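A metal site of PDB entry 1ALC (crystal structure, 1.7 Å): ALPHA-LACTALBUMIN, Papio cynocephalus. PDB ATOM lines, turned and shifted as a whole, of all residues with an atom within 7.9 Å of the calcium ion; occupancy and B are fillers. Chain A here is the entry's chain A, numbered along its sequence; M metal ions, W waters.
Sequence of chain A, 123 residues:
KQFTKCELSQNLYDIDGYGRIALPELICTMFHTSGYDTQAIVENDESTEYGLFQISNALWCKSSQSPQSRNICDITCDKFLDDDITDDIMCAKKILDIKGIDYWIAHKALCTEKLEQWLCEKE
Five residues have an atom within 4 Å of the calcium ion: Lys 79, Asp 82, Asp 84, Asp 87 and Asp 88.
Water W2 lies within hydrogen-bond range of O of Asp 82 (2.7 Å) and OD2 of Asp 88 (3.2 Å). Water W1 lies within hydrogen-bond range of the side-chain carboxylate (OD2) of Asp 87 (2.5 Å) and the side-chain carboxylate (OD2) of Asp 82 (2.8 Å).
The calcium ion is bound by O of Lys 79 (2.2 Å), O of Asp 84 (2.3 Å), OD1 of Asp 88 (2.3 Å), OD1 of Asp 87 (2.3 Å), OD1 of Asp 82 (2.4 Å), water W2 (2.4 Å) and water W1 (2.6 Å).
The side-chain carboxylate of Asp 84 lies within hydrogen-bond range of the side-chain hydroxyl of Thr 86 (2.6 Å).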
ATOM      1  N   THR A  38       2.748 -22.487  15.125  1.00  0.00           N
ATOM      2  CA  THR A  38       1.978 -22.882  16.281  1.00  0.00           C
ATOM      3  C   THR A  38       2.270 -24.312  16.708  1.00  0.00           C
ATOM      4  O   THR A  38       1.885 -24.674  17.818  1.00  0.00           O
ATOM      5  CB  THR A  38       0.404 -22.734  16.089  1.00  0.00           C
ATOM      6  OG1 THR A  38       0.087 -23.763  15.084  1.00  0.00           O
ATOM      7  CG2 THR A  38      -0.052 -21.338  15.631  1.00  0.00           C
ATOM      8  N   ILE A  75      -2.214 -25.237  32.749  1.00  0.00           N
ATOM      9  CA  ILE A  75      -2.805 -25.803  31.496  1.00  0.00           C
ATOM     10  C   ILE A  75      -1.910 -26.917  30.951  1.00  0.00           C
ATOM     11  O   ILE A  75      -0.695 -26.957  31.242  1.00  0.00           O
ATOM     12  CB  ILE A  75      -3.028 -24.642  30.490  1.00  0.00           C
ATOM     13  CG1 ILE A  75      -3.781 -25.196  29.217  1.00  0.00           C
ATOM     14  CG2 ILE A  75      -1.718 -23.919  30.090  1.00  0.00           C
ATOM     15  CD1 ILE A  75      -4.003 -24.087  28.144  1.00  0.00           C
ATOM     16  N   THR A  76      -2.580 -27.778  30.187  1.00  0.00           N
ATOM     17  CA  THR A  76      -1.830 -28.913  29.558  1.00  0.00           C
ATOM     18  C   THR A  76      -1.079 -28.304  28.387  1.00  0.00           C
ATOM     19  O   THR A  76      -1.661 -27.492  27.630  1.00  0.00           O
ATOM     20  CB  THR A  76      -2.808 -30.055  29.106  1.00  0.00           C
ATOM     21  OG1 THR A  76      -2.034 -30.852  28.116  1.00  0.00           O
ATOM     22  CG2 THR A  76      -4.075 -29.546  28.423  1.00  0.00           C
ATOM     23  N   CYS A  77       0.176 -28.667  28.204  1.00  0.00           N
ATOM     24  CA  CYS A  77       1.022 -28.183  27.132  1.00  0.00           C
ATOM     25  C   CYS A  77       0.408 -28.465  25.720  1.00  0.00           C
ATOM     26  O   CYS A  77       0.964 -27.836  24.836  1.00  0.00           O
ATOM     27  CB  CYS A  77       2.433 -28.785  27.074  1.00  0.00           C
ATOM     28  SG  CYS A  77       3.343 -28.541  28.664  1.00  0.00           S
ATOM     29  N   ASP A  78      -0.533 -29.372  25.705  1.00  0.00           N
ATOM     30  CA  ASP A  78      -1.129 -29.735  24.374  1.00  0.00           C
ATOM     31  C   ASP A  78      -1.901 -28.559  23.797  1.00  0.00           C
ATOM     32  O   ASP A  78      -2.092 -28.453  22.573  1.00  0.00           O
ATOM     33  CB  ASP A  78      -1.950 -31.005  24.481  1.00  0.00           C
ATOM     34  CG  ASP A  78      -3.411 -30.826  24.813  1.00  0.00           C
ATOM     35  OD1 ASP A  78      -3.826 -31.039  25.959  1.00  0.00           O
ATOM     36  OD2 ASP A  78      -4.181 -30.466  23.886  1.00  0.00           O
ATOM     37  N   LYS A  79      -2.357 -27.733  24.707  1.00  0.00           N
ATOM     38  CA  LYS A  79      -3.160 -26.533  24.334  1.00  0.00           C
ATOM     39  C   LYS A  79      -2.346 -25.522  23.586  1.00  0.00           C
ATOM     40  O   LYS A  79      -2.933 -24.595  22.919  1.00  0.00           O
ATOM     41  CB  LYS A  79      -3.792 -25.957  25.624  1.00  0.00           C
ATOM     42  CG  LYS A  79      -4.763 -26.937  26.283  1.00  0.00           C
ATOM     43  CD  LYS A  79      -5.867 -27.371  25.350  1.00  0.00           C
ATOM     44  CE  LYS A  79      -6.706 -26.175  24.873  1.00  0.00           C
ATOM     45  NZ  LYS A  79      -8.138 -26.588  24.895  1.00  0.00           N
ATOM     46  N   PHE A  80      -1.041 -25.616  23.598  1.00  0.00           N
ATOM     47  CA  PHE A  80      -0.112 -24.706  22.894  1.00  0.00           C
ATOM     48  C   PHE A  80       0.212 -25.161  21.488  1.00  0.00           C
ATOM     49  O   PHE A  80       1.076 -24.547  20.807  1.00  0.00           O
ATOM     50  CB  PHE A  80       1.121 -24.363  23.730  1.00  0.00           C
ATOM     51  CG  PHE A  80       0.733 -23.695  25.032  1.00  0.00           C
ATOM     52  CD1 PHE A  80       1.614 -23.675  26.114  1.00  0.00           C
ATOM     53  CD2 PHE A  80      -0.521 -23.094  25.146  1.00  0.00           C
ATOM     54  CE1 PHE A  80       1.269 -23.045  27.294  1.00  0.00           C
ATOM     55  CE2 PHE A  80      -0.904 -22.490  26.346  1.00  0.00           C
ATOM     56  CZ  PHE A  80       0.001 -22.467  27.426  1.00  0.00           C
ATOM     57  N   LEU A  81      -0.462 -26.201  21.051  1.00  0.00           N
ATOM     58  CA  LEU A  81      -0.246 -26.818  19.733  1.00  0.00           C
ATOM     59  C   LEU A  81      -1.427 -26.724  18.800  1.00  0.00           C
ATOM     60  O   LEU A  81      -1.308 -27.307  17.697  1.00  0.00           O
ATOM     61  CB  LEU A  81       0.195 -28.283  20.020  1.00  0.00           C
ATOM     62  CG  LEU A  81       1.402 -28.384  20.940  1.00  0.00           C
ATOM     63  CD1 LEU A  81       1.641 -29.787  21.427  1.00  0.00           C
ATOM     64  CD2 LEU A  81       2.633 -27.820  20.224  1.00  0.00           C
ATOM     65  N   ASP A  82      -2.476 -26.053  19.257  1.00  0.00           N
ATOM     66  CA  ASP A  82      -3.700 -25.914  18.378  1.00  0.00           C
ATOM     67  C   ASP A  82      -3.649 -24.601  17.626  1.00  0.00           C
ATOM     68  O   ASP A  82      -2.671 -23.824  17.725  1.00  0.00           O
ATOM     69  CB  ASP A  82      -4.925 -26.299  19.135  1.00  0.00           C
ATOM     70  CG  ASP A  82      -5.107 -25.383  20.399  1.00  0.00           C
ATOM     71  OD1 ASP A  82      -4.411 -24.380  20.390  1.00  0.00           O
ATOM     72  OD2 ASP A  82      -5.903 -25.793  21.200  1.00  0.00           O
ATOM     73  N   ASP A  83      -4.706 -24.354  16.808  1.00  0.00           N
ATOM     74  CA  ASP A  83      -4.785 -23.151  15.987  1.00  0.00           C
ATOM     75  C   ASP A  83      -5.459 -21.967  16.678  1.00  0.00           C
ATOM     76  O   ASP A  83      -5.809 -20.953  16.027  1.00  0.00           O
ATOM     77  CB  ASP A  83      -5.047 -23.335  14.523  1.00  0.00           C
ATOM     78  CG  ASP A  83      -6.260 -23.992  13.959  1.00  0.00           C
ATOM     79  OD1 ASP A  83      -6.168 -24.455  12.779  1.00  0.00           O
ATOM     80  OD2 ASP A  83      -7.343 -24.099  14.564  1.00  0.00           O
ATOM     81  N   ASP A  84      -5.588 -22.079  17.982  1.00  0.00           N
ATOM     82  CA  ASP A  84      -6.187 -20.965  18.782  1.00  0.00           C
ATOM     83  C   ASP A  84      -5.030 -20.481  19.677  1.00  0.00           C
ATOM     84  O   ASP A  84      -4.747 -21.256  20.615  1.00  0.00           O
ATOM     85  CB  ASP A  84      -7.404 -21.371  19.501  1.00  0.00           C
ATOM     86  CG  ASP A  84      -8.053 -20.188  20.291  1.00  0.00           C
ATOM     87  OD1 ASP A  84      -8.874 -20.440  21.147  1.00  0.00           O
ATOM     88  OD2 ASP A  84      -7.678 -19.060  19.938  1.00  0.00           O
ATOM     89  N   ILE A  85      -4.436 -19.370  19.349  1.00  0.00           N
ATOM     90  CA  ILE A  85      -3.342 -18.849  20.196  1.00  0.00           C
ATOM     91  C   ILE A  85      -3.862 -18.016  21.351  1.00  0.00           C
ATOM     92  O   ILE A  85      -3.004 -17.359  22.035  1.00  0.00           O
ATOM     93  CB  ILE A  85      -2.266 -18.118  19.366  1.00  0.00           C
ATOM     94  CG1 ILE A  85      -2.872 -16.852  18.694  1.00  0.00           C
ATOM     95  CG2 ILE A  85      -1.585 -19.028  18.300  1.00  0.00           C
ATOM     96  CD1 ILE A  85      -1.829 -15.865  18.111  1.00  0.00           C
ATOM     97  N   THR A  86      -5.160 -18.044  21.604  1.00  0.00           N
ATOM     98  CA  THR A  86      -5.708 -17.252  22.727  1.00  0.00           C
ATOM     99  C   THR A  86      -5.061 -17.675  24.052  1.00  0.00           C
ATOM    100  O   THR A  86      -4.450 -16.816  24.745  1.00  0.00           O
ATOM    101  CB  THR A  86      -7.272 -17.242  22.866  1.00  0.00           C
ATOM    102  OG1 THR A  86      -7.813 -16.982  21.536  1.00  0.00           O
ATOM    103  CG2 THR A  86      -7.794 -16.213  23.886  1.00  0.00           C
ATOM    104  N   ASP A  87      -5.229 -18.937  24.404  1.00  0.00           N
ATOM    105  CA  ASP A  87      -4.687 -19.491  25.659  1.00  0.00           C
ATOM    106  C   ASP A  87      -3.186 -19.233  25.749  1.00  0.00           C
ATOM    107  O   ASP A  87      -2.653 -18.873  26.821  1.00  0.00           O
ATOM    108  CB  ASP A  87      -5.113 -20.904  25.973  1.00  0.00           C
ATOM    109  CG  ASP A  87      -5.093 -21.865  24.767  1.00  0.00           C
ATOM    110  OD1 ASP A  87      -4.471 -21.542  23.764  1.00  0.00           O
ATOM    111  OD2 ASP A  87      -5.738 -22.918  24.941  1.00  0.00           O
ATOM    112  N   ASP A  88      -2.518 -19.452  24.639  1.00  0.00           N
ATOM    113  CA  ASP A  88      -1.088 -19.251  24.486  1.00  0.00           C
ATOM    114  C   ASP A  88      -0.728 -17.840  24.997  1.00  0.00           C
ATOM    115  O   ASP A  88       0.209 -17.620  25.780  1.00  0.00           O
ATOM    116  CB  ASP A  88      -0.629 -19.386  23.020  1.00  0.00           C
ATOM    117  CG  ASP A  88      -0.898 -20.757  22.408  1.00  0.00           C
ATOM    118  OD1 ASP A  88      -2.014 -21.271  22.486  1.00  0.00           O
ATOM    119  OD2 ASP A  88       0.112 -21.299  21.913  1.00  0.00           O
ATOM    120  N   ILE A  89      -1.533 -16.904  24.426  1.00  0.00           N
ATOM    121  CA  ILE A  89      -1.360 -15.496  24.740  1.00  0.00           C
ATOM    122  C   ILE A  89      -1.549 -15.236  26.237  1.00  0.00           C
ATOM    123  O   ILE A  89      -0.800 -14.391  26.773  1.00  0.00           O
ATOM    124  CB  ILE A  89      -2.297 -14.580  23.879  1.00  0.00           C
ATOM    125  CG1 ILE A  89      -1.671 -14.440  22.461  1.00  0.00           C
ATOM    126  CG2 ILE A  89      -2.417 -13.179  24.561  1.00  0.00           C
ATOM    127  CD1 ILE A  89      -2.606 -13.788  21.412  1.00  0.00           C
HETATM  128 CA    CA M   1      -3.685 -22.749  21.946  1.00  0.00          CA
HETATM  129  O   HOH W   1      -6.147 -23.371  22.492  1.00  0.00           O
HETATM  130  O   HOH W   2      -2.069 -22.913  20.152  1.00  0.00           O
